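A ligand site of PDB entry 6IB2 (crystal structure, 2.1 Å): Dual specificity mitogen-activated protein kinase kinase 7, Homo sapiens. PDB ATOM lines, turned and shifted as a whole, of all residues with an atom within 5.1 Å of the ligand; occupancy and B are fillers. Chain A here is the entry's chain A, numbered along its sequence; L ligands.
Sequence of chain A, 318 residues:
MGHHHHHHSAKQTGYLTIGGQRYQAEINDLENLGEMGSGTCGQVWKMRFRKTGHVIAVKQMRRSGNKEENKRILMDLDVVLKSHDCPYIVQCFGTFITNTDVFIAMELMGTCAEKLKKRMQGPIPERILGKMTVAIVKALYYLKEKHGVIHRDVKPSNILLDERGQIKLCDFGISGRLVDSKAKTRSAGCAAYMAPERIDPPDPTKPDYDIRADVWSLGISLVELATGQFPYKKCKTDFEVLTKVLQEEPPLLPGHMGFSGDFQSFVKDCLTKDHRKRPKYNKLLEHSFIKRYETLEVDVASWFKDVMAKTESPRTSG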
ATOM      1  N   MET A  36     -13.960 -15.129 -10.553  1.00  0.00           N
ATOM      2  CA  MET A  36     -13.088 -14.311 -11.377  1.00  0.00           C
ATOM      3  C   MET A  36     -12.897 -15.005 -12.719  1.00  0.00           C
ATOM      4  O   MET A  36     -12.321 -16.096 -12.782  1.00  0.00           O
ATOM      5  CB  MET A  36     -11.737 -14.073 -10.699  1.00  0.00           C
ATOM      6  CG  MET A  36     -11.840 -13.425  -9.336  1.00  0.00           C
ATOM      7  SD  MET A  36     -10.228 -12.945  -8.674  1.00  0.00           S
ATOM      8  CE  MET A  36      -9.361 -14.508  -8.754  1.00  0.00           C
ATOM      9  N   GLY A  37     -13.371 -14.374 -13.787  1.00  0.00           N
ATOM     10  CA  GLY A  37     -13.242 -14.913 -15.129  1.00  0.00           C
ATOM     11  C   GLY A  37     -13.940 -16.246 -15.314  1.00  0.00           C
ATOM     12  O   GLY A  37     -14.665 -16.448 -16.292  1.00  0.00           O
ATOM     13  N   VAL A  44     -11.870 -20.011 -10.595  1.00  0.00           N
ATOM     14  CA  VAL A  44     -11.040 -19.372  -9.568  1.00  0.00           C
ATOM     15  C   VAL A  44     -11.899 -18.361  -8.826  1.00  0.00           C
ATOM     16  O   VAL A  44     -12.441 -17.433  -9.434  1.00  0.00           O
ATOM     17  CB  VAL A  44      -9.803 -18.700 -10.179  1.00  0.00           C
ATOM     18  CG1 VAL A  44      -8.915 -18.135  -9.085  1.00  0.00           C
ATOM     19  CG2 VAL A  44      -9.031 -19.683 -11.041  1.00  0.00           C
ATOM     20  N   ALA A  57      -6.959 -15.428  -4.052  1.00  0.00           N
ATOM     21  CA  ALA A  57      -7.557 -16.189  -5.135  1.00  0.00           C
ATOM     22  C   ALA A  57      -7.604 -17.661  -4.741  1.00  0.00           C
ATOM     23  O   ALA A  57      -6.598 -18.205  -4.260  1.00  0.00           O
ATOM     24  CB  ALA A  57      -6.791 -16.004  -6.441  1.00  0.00           C
ATOM     25  N   LYS A  59      -8.750 -21.486  -6.107  1.00  0.00           N
ATOM     26  CA  LYS A  59      -9.180 -22.419  -7.150  1.00  0.00           C
ATOM     27  C   LYS A  59      -9.814 -23.637  -6.485  1.00  0.00           C
ATOM     28  O   LYS A  59      -9.225 -24.228  -5.570  1.00  0.00           O
ATOM     29  CB  LYS A  59      -8.013 -22.837  -8.035  1.00  0.00           C
ATOM     30  CG  LYS A  59      -8.284 -24.077  -8.875  1.00  0.00           C
ATOM     31  CD  LYS A  59      -7.145 -24.365  -9.831  1.00  0.00           C
ATOM     32  CE  LYS A  59      -7.218 -23.489 -11.068  1.00  0.00           C
ATOM     33  NZ  LYS A  59      -8.412 -23.810 -11.904  1.00  0.00           N
ATOM     34  N   ARG A  72      -4.561 -32.690 -14.370  1.00  0.00           N
ATOM     35  CA  ARG A  72      -3.611 -31.615 -14.651  1.00  0.00           C
ATOM     36  C   ARG A  72      -3.546 -30.598 -13.528  1.00  0.00           C
ATOM     37  O   ARG A  72      -2.495 -29.979 -13.321  1.00  0.00           O
ATOM     38  CB  ARG A  72      -3.973 -30.932 -15.974  1.00  0.00           C
ATOM     39  N   ILE A  73      -4.655 -30.385 -12.807  1.00  0.00           N
ATOM     40  CA  ILE A  73      -4.651 -29.430 -11.709  1.00  0.00           C
ATOM     41  C   ILE A  73      -3.732 -29.911 -10.585  1.00  0.00           C
ATOM     42  O   ILE A  73      -2.968 -29.119 -10.017  1.00  0.00           O
ATOM     43  CB  ILE A  73      -6.089 -29.190 -11.201  1.00  0.00           C
ATOM     44  CG1 ILE A  73      -6.883 -28.390 -12.233  1.00  0.00           C
ATOM     45  CG2 ILE A  73      -6.081 -28.483  -9.855  1.00  0.00           C
ATOM     46  CD1 ILE A  73      -8.303 -28.080 -11.804  1.00  0.00           C
ATOM     47  N   ASP A  76       0.005 -29.440 -11.915  1.00  0.00           N
ATOM     48  CA  ASP A  76       0.553 -28.084 -11.873  1.00  0.00           C
ATOM     49  C   ASP A  76       0.719 -27.606 -10.435  1.00  0.00           C
ATOM     50  O   ASP A  76       1.692 -26.908 -10.117  1.00  0.00           O
ATOM     51  CB  ASP A  76      -0.346 -27.133 -12.656  1.00  0.00           C
ATOM     52  CG  ASP A  76      -0.454 -27.503 -14.116  1.00  0.00           C
ATOM     53  OD1 ASP A  76       0.184 -28.485 -14.533  1.00  0.00           O
ATOM     54  OD2 ASP A  76      -1.200 -26.818 -14.847  1.00  0.00           O
ATOM     55  N   LEU A  77      -0.210 -27.970  -9.546  1.00  0.00           N
ATOM     56  CA  LEU A  77      -0.077 -27.628  -8.143  1.00  0.00           C
ATOM     57  C   LEU A  77       1.216 -28.183  -7.562  1.00  0.00           C
ATOM     58  O   LEU A  77       1.863 -27.547  -6.724  1.00  0.00           O
ATOM     59  CB  LEU A  77      -1.279 -28.134  -7.351  1.00  0.00           C
ATOM     60  CG  LEU A  77      -1.190 -28.049  -5.825  1.00  0.00           C
ATOM     61  CD1 LEU A  77      -0.986 -26.604  -5.372  1.00  0.00           C
ATOM     62  CD2 LEU A  77      -2.430 -28.649  -5.173  1.00  0.00           C
ATOM     63  N   VAL A  80       3.649 -25.728  -8.685  1.00  0.00           N
ATOM     64  CA  VAL A  80       3.445 -24.455  -7.985  1.00  0.00           C
ATOM     65  C   VAL A  80       4.012 -24.529  -6.575  1.00  0.00           C
ATOM     66  O   VAL A  80       4.692 -23.596  -6.115  1.00  0.00           O
ATOM     67  CB  VAL A  80       1.948 -24.085  -7.981  1.00  0.00           C
ATOM     68  CG1 VAL A  80       1.705 -22.881  -7.084  1.00  0.00           C
ATOM     69  CG2 VAL A  80       1.459 -23.801  -9.390  1.00  0.00           C
ATOM     70  N   VAL A  90       3.111 -17.362  -9.907  1.00  0.00           N
ATOM     71  CA  VAL A  90       2.067 -17.162  -8.907  1.00  0.00           C
ATOM     72  C   VAL A  90       2.259 -18.152  -7.766  1.00  0.00           C
ATOM     73  O   VAL A  90       2.406 -19.357  -7.981  1.00  0.00           O
ATOM     74  CB  VAL A  90       0.682 -17.287  -9.552  1.00  0.00           C
ATOM     75  CG1 VAL A  90       0.364 -16.044 -10.362  1.00  0.00           C
ATOM     76  CG2 VAL A  90       0.600 -18.530 -10.420  1.00  0.00           C
ATOM     77  N   ILE A 104      -7.474 -24.527  -3.440  1.00  0.00           N
ATOM     78  CA  ILE A 104      -6.074 -24.128  -3.558  1.00  0.00           C
ATOM     79  C   ILE A 104      -6.022 -22.610  -3.448  1.00  0.00           C
ATOM     80  O   ILE A 104      -6.443 -21.894  -4.364  1.00  0.00           O
ATOM     81  CB  ILE A 104      -5.453 -24.613  -4.881  1.00  0.00           C
ATOM     82  CG1 ILE A 104      -5.999 -25.981  -5.257  1.00  0.00           C
ATOM     83  CG2 ILE A 104      -3.947 -24.680  -4.740  1.00  0.00           C
ATOM     84  CD1 ILE A 104      -5.501 -26.484  -6.595  1.00  0.00           C
ATOM     85  N   MET A 106      -4.377 -19.142  -3.707  1.00  0.00           N
ATOM     86  CA  MET A 106      -3.331 -18.607  -4.554  1.00  0.00           C
ATOM     87  C   MET A 106      -3.181 -17.111  -4.319  1.00  0.00           C
ATOM     88  O   MET A 106      -4.109 -16.424  -3.868  1.00  0.00           O
ATOM     89  CB  MET A 106      -3.642 -18.864  -6.035  1.00  0.00           C
ATOM     90  CG  MET A 106      -2.399 -19.115  -6.880  1.00  0.00           C
ATOM     91  SD  MET A 106      -1.626 -20.683  -6.457  1.00  0.00           S
ATOM     92  CE  MET A 106      -3.017 -21.783  -6.572  1.00  0.00           C
ATOM     93  N   GLU A 107      -1.989 -16.611  -4.634  1.00  0.00           N
ATOM     94  CA  GLU A 107      -1.720 -15.186  -4.579  1.00  0.00           C
ATOM     95  C   GLU A 107      -2.615 -14.430  -5.561  1.00  0.00           C
ATOM     96  O   GLU A 107      -2.634 -14.740  -6.753  1.00  0.00           O
ATOM     97  CB  GLU A 107      -0.241 -14.924  -4.891  1.00  0.00           C
ATOM     98  CG  GLU A 107       0.070 -13.542  -5.413  1.00  0.00           C
ATOM     99  CD  GLU A 107       1.527 -13.399  -5.811  1.00  0.00           C
ATOM    100  OE1 GLU A 107       2.122 -12.343  -5.522  1.00  0.00           O
ATOM    101  OE2 GLU A 107       2.071 -14.350  -6.402  1.00  0.00           O
ATOM    102  N   LEU A 108      -3.353 -13.451  -5.050  1.00  0.00           N
ATOM    103  CA  LEU A 108      -4.304 -12.714  -5.863  1.00  0.00           C
ATOM    104  C   LEU A 108      -3.585 -11.655  -6.684  1.00  0.00           C
ATOM    105  O   LEU A 108      -2.956 -10.752  -6.119  1.00  0.00           O
ATOM    106  CB  LEU A 108      -5.381 -12.072  -4.981  1.00  0.00           C
ATOM    107  CG  LEU A 108      -6.467 -11.306  -5.743  1.00  0.00           C
ATOM    108  CD1 LEU A 108      -7.365 -12.270  -6.495  1.00  0.00           C
ATOM    109  CD2 LEU A 108      -7.274 -10.444  -4.793  1.00  0.00           C
ATOM    110  N   MET A 109      -3.675 -11.757  -8.001  1.00  0.00           N
ATOM    111  CA  MET A 109      -3.107 -10.784  -8.918  1.00  0.00           C
ATOM    112  C   MET A 109      -4.192  -9.807  -9.373  1.00  0.00           C
ATOM    113  O   MET A 109      -5.371  -9.931  -9.029  1.00  0.00           O
ATOM    114  CB  MET A 109      -2.447 -11.485 -10.100  1.00  0.00           C
ATOM    115  CG  MET A 109      -1.350 -12.471  -9.725  1.00  0.00           C
ATOM    116  SD  MET A 109       0.106 -11.691  -9.022  1.00  0.00           S
ATOM    117  CE  MET A 109       0.720 -10.764 -10.426  1.00  0.00           C
ATOM    118  N   GLY A 110      -3.791  -8.822 -10.167  1.00  0.00           N
ATOM    119  CA  GLY A 110      -4.726  -7.851 -10.688  1.00  0.00           C
ATOM    120  C   GLY A 110      -5.508  -8.363 -11.879  1.00  0.00           C
ATOM    121  O   GLY A 110      -6.715  -8.589 -11.801  1.00  0.00           O
ATOM    122  N   CYS A 112      -4.789 -10.250 -16.219  1.00  0.00           N
ATOM    123  CA  CYS A 112      -3.863 -10.832 -17.176  1.00  0.00           C
ATOM    124  C   CYS A 112      -3.510  -9.812 -18.264  1.00  0.00           C
ATOM    125  O   CYS A 112      -4.132  -8.755 -18.395  1.00  0.00           O
ATOM    126  CB  CYS A 112      -4.450 -12.097 -17.788  1.00  0.00           C
ATOM    127  SG  CYS A 112      -5.658 -11.814 -19.095  1.00  0.00           S
ATOM    128  N   ALA A 113      -2.495 -10.157 -19.055  1.00  0.00           N
ATOM    129  CA  ALA A 113      -2.017  -9.250 -20.089  1.00  0.00           C
ATOM    130  C   ALA A 113      -3.024  -9.113 -21.226  1.00  0.00           C
ATOM    131  O   ALA A 113      -3.051  -8.068 -21.897  1.00  0.00           O
ATOM    132  CB  ALA A 113      -0.666  -9.715 -20.631  1.00  0.00           C
ATOM    133  N   GLU A 114      -3.847 -10.134 -21.457  1.00  0.00           N
ATOM    134  CA  GLU A 114      -4.853 -10.041 -22.511  1.00  0.00           C
ATOM    135  C   GLU A 114      -5.937  -9.025 -22.143  1.00  0.00           C
ATOM    136  O   GLU A 114      -6.413  -8.281 -22.996  1.00  0.00           O
ATOM    137  CB  GLU A 114      -5.466 -11.410 -22.777  1.00  0.00           C
ATOM    138  CG  GLU A 114      -6.544 -11.410 -23.845  1.00  0.00           C
ATOM    139  CD  GLU A 114      -6.911 -12.805 -24.309  1.00  0.00           C
ATOM    140  OE1 GLU A 114      -6.040 -13.705 -24.277  1.00  0.00           O
ATOM    141  OE2 GLU A 114      -8.090 -13.013 -24.703  1.00  0.00           O
ATOM    142  N   LYS A 115      -6.340  -8.995 -20.861  1.00  0.00           N
ATOM    143  CA  LYS A 115      -7.302  -7.985 -20.425  1.00  0.00           C
ATOM    144  C   LYS A 115      -6.676  -6.595 -20.445  1.00  0.00           C
ATOM    145  O   LYS A 115      -7.367  -5.611 -20.740  1.00  0.00           O
ATOM    146  CB  LYS A 115      -7.827  -8.326 -19.036  1.00  0.00           C
ATOM    147  CG  LYS A 115      -8.449  -9.700 -18.909  1.00  0.00           C
ATOM    148  CD  LYS A 115      -9.684  -9.854 -19.777  1.00  0.00           C
ATOM    149  CE  LYS A 115     -10.304 -11.229 -19.604  1.00  0.00           C
ATOM    150  NZ  LYS A 115     -11.538 -11.398 -20.430  1.00  0.00           N
ATOM    151  N   PRO A 156      -0.566 -14.183 -23.745  1.00  0.00           N
ATOM    152  CA  PRO A 156      -0.911 -13.065 -22.844  1.00  0.00           C
ATOM    153  C   PRO A 156      -1.908 -13.430 -21.763  1.00  0.00           C
ATOM    154  O   PRO A 156      -1.937 -12.758 -20.721  1.00  0.00           O
ATOM    155  CB  PRO A 156      -1.479 -12.015 -23.799  1.00  0.00           C
ATOM    156  CG  PRO A 156      -0.801 -12.293 -25.097  1.00  0.00           C
ATOM    157  CD  PRO A 156      -0.673 -13.782 -25.164  1.00  0.00           C
ATOM    158  N   SER A 157      -2.740 -14.462 -21.967  1.00  0.00           N
ATOM    159  CA  SER A 157      -3.669 -14.876 -20.924  1.00  0.00           C
ATOM    160  C   SER A 157      -2.973 -15.537 -19.744  1.00  0.00           C
ATOM    161  O   SER A 157      -3.561 -15.609 -18.660  1.00  0.00           O
ATOM    162  CB  SER A 157      -4.724 -15.822 -21.509  1.00  0.00           C
ATOM    163  OG  SER A 157      -4.128 -16.987 -22.049  1.00  0.00           O
ATOM    164  N   LEU A 160       0.293 -12.627 -15.741  1.00  0.00           N
ATOM    165  CA  LEU A 160      -0.496 -11.910 -14.752  1.00  0.00           C
ATOM    166  C   LEU A 160       0.272 -10.711 -14.213  1.00  0.00           C
ATOM    167  O   LEU A 160       1.499 -10.766 -14.060  1.00  0.00           O
ATOM    168  CB  LEU A 160      -0.898 -12.832 -13.589  1.00  0.00           C
ATOM    169  CG  LEU A 160      -1.812 -14.004 -13.942  1.00  0.00           C
ATOM    170  CD1 LEU A 160      -2.202 -14.764 -12.679  1.00  0.00           C
ATOM    171  CD2 LEU A 160      -3.048 -13.526 -14.680  1.00  0.00           C
ATOM    172  N   CYS A 170       1.207 -17.550 -14.949  1.00  0.00           N
ATOM    173  CA  CYS A 170       0.007 -18.108 -14.311  1.00  0.00           C
ATOM    174  C   CYS A 170      -0.026 -19.624 -14.360  1.00  0.00           C
ATOM    175  O   CYS A 170       0.217 -20.299 -13.355  1.00  0.00           O
ATOM    176  CB  CYS A 170      -1.241 -17.507 -14.968  1.00  0.00           C
ATOM    177  SG  CYS A 170      -2.792 -18.297 -14.495  1.00  0.00           S
ATOM    178  N   ASP A 171      -0.343 -20.183 -15.528  1.00  0.00           N
ATOM    179  CA  ASP A 171      -0.603 -21.605 -15.682  1.00  0.00           C
ATOM    180  C   ASP A 171       0.532 -22.274 -16.438  1.00  0.00           C
ATOM    181  O   ASP A 171       1.340 -21.626 -17.098  1.00  0.00           O
ATOM    182  CB  ASP A 171      -1.939 -21.838 -16.391  1.00  0.00           C
ATOM    183  CG  ASP A 171      -2.563 -23.171 -16.053  1.00  0.00           C
ATOM    184  OD1 ASP A 171      -1.810 -24.152 -15.876  1.00  0.00           O
ATOM    185  OD2 ASP A 171      -3.805 -23.241 -15.942  1.00  0.00           O
HETATM  186  N1  LIG L   1      -5.099 -13.557  -9.293  1.00  0.00           N
HETATM  187  C1  LIG L   1      -5.964 -12.876 -10.074  1.00  0.00           C
HETATM  188  O1  LIG L   1      -2.752 -26.135 -10.679  1.00  0.00           O
HETATM  189  C2  LIG L   1      -6.295 -14.664 -11.567  1.00  0.00           C
HETATM  190  C3  LIG L   1      -3.419 -23.994 -11.366  1.00  0.00           C
HETATM  191  C4  LIG L   1      -3.034 -23.384 -10.192  1.00  0.00           C
HETATM  192  C5  LIG L   1      -3.178 -22.009 -10.047  1.00  0.00           C
HETATM  193  C6  LIG L   1      -3.275 -25.478 -11.547  1.00  0.00           C
HETATM  194  C7  LIG L   1      -3.804 -26.082 -12.813  1.00  0.00           C
HETATM  195  C8  LIG L   1      -7.627 -15.223 -13.710  1.00  0.00           C
HETATM  196  C9  LIG L   1      -8.864 -16.096 -13.546  1.00  0.00           C
HETATM  197  C10 LIG L   1      -9.801 -15.928 -14.730  1.00  0.00           C
HETATM  198  C11 LIG L   1      -9.089 -16.227 -16.041  1.00  0.00           C
HETATM  199  C12 LIG L   1      -6.939 -15.599 -15.024  1.00  0.00           C
HETATM  200  C13 LIG L   1      -5.361 -15.456 -10.758  1.00  0.00           C
HETATM  201  C14 LIG L   1      -7.775 -14.394 -16.968  1.00  0.00           C
HETATM  202  C15 LIG L   1      -6.388 -14.248 -17.559  1.00  0.00           C
HETATM  203  C16 LIG L   1      -6.435 -13.267 -18.705  1.00  0.00           C
HETATM  204  C17 LIG L   1      -4.750 -14.839  -9.561  1.00  0.00           C
HETATM  205  C18 LIG L   1      -5.338 -16.748 -11.474  1.00  0.00           C
HETATM  206  C19 LIG L   1      -4.528 -17.915 -11.054  1.00  0.00           C
HETATM  207  C20 LIG L   1      -4.785 -19.188 -11.519  1.00  0.00           C
HETATM  208  C21 LIG L   1      -3.693 -21.192 -11.049  1.00  0.00           C
HETATM  209  C22 LIG L   1      -4.059 -21.846 -12.221  1.00  0.00           C
HETATM  210  C23 LIG L   1      -3.930 -23.216 -12.392  1.00  0.00           C
HETATM  211  N2  LIG L   1      -6.549 -13.389 -11.180  1.00  0.00           N
HETATM  212  N3  LIG L   1      -6.703 -15.453 -12.579  1.00  0.00           N
HETATM  213  N4  LIG L   1      -6.135 -16.746 -12.553  1.00  0.00           N
HETATM  214  N5  LIG L   1      -3.873 -15.515  -8.774  1.00  0.00           N
HETATM  215  N6  LIG L   1      -3.825 -19.869 -10.900  1.00  0.00           N
HETATM  216  N7  LIG L   1      -2.980 -19.114 -10.081  1.00  0.00           N
HETATM  217  N8  LIG L   1      -3.469 -17.801 -10.208  1.00  0.00           N
HETATM  218  N9  LIG L   1      -7.922 -15.354 -16.058  1.00  0.00           N
HETATM  219  O2  LIG L   1      -8.674 -13.657 -17.326  1.00  0.00           O
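O of Ile 73 lies close to O1 of the ligand.
Met 36 touches the ligand.
CA of Gly 37 touches C10 of the ligand, at 3.6 Å.
Ala 57 touches the ligand.
CE of Lys 59 touches C23 of the ligand, at 3.6 Å.
CB of Asp 76 touches O1 of the ligand (3.3 Å).
Val 90 touches the ligand (CG2 to N7, 3.6 Å).
CG of Met 106 touches N7 of the ligand, 3.3 Å away.
Leu 108 touches the ligand.
CE of Lys 115 touches O2 of the ligand, at 3.7 Å.
O of Ser 157 touches C15 of the ligand, 3.3 Å away.
CD1 of Leu 160 touches C13 of the ligand, 3.8 Å away.
Cys 170 touches the ligand (SG to C20, 3.7 Å).
Asp 171 touches the ligand (OD2 to C23, 3.6 Å).
Hydrophobic or aromatic side chains that line the ligand: Met 36, Ala 57, Ile 73, Val 90, Met 106, Leu 108, Met 109 and Leu 160.
18 residues have an atom within 4 Å of the ligand: Met 36, Gly 37, Ala 57, Lys 59, Ile 73, Asp 76, Leu 77, Val 90, Met 106, Glu 107, Leu 108, Met 109, Cys 112, Lys 115, Ser 157, Leu 160, Cys 170 and Asp 171.
Along chain A the residues within 4 Å of the ligand span positions 36 to 171.
N of Met 109 lies within hydrogen-bond range of N1 of the ligand (2.6 Å).
The backbone carbonyl oxygen (O) of Glu 107 sits at hydrogen-bond distance from a nitrogen (N5) of the ligand.
The side-chain sulfur of Cys 112 is bonded to a carbon (C16) of the ligand, at 1.7 Å.
O1 of the ligand is in hydrogen-bond range of N of Leu 77 (3.3 Å).
The backbone NH (N) of Lys 115 is in hydrogen-bond range of the side-chain sulfur (SG) of Cys 112, 3.4 Å away.
The backbone NH of Met 106 is in hydrogen-bond range of the backbone carbonyl oxygen of Ala 57 (2.5 Å).
The side-chain sulfur (SG) of Cys 112 sits close to the backbone NH (N) of Glu 114 (3.4 Å).
O of Val 44 lies within hydrogen-bond range of N of Met 36 (3.0 Å).
The backbone carbonyl oxygen (O) of Lys 59 is in hydrogen-bond range of the backbone NH (N) of Ile 104.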
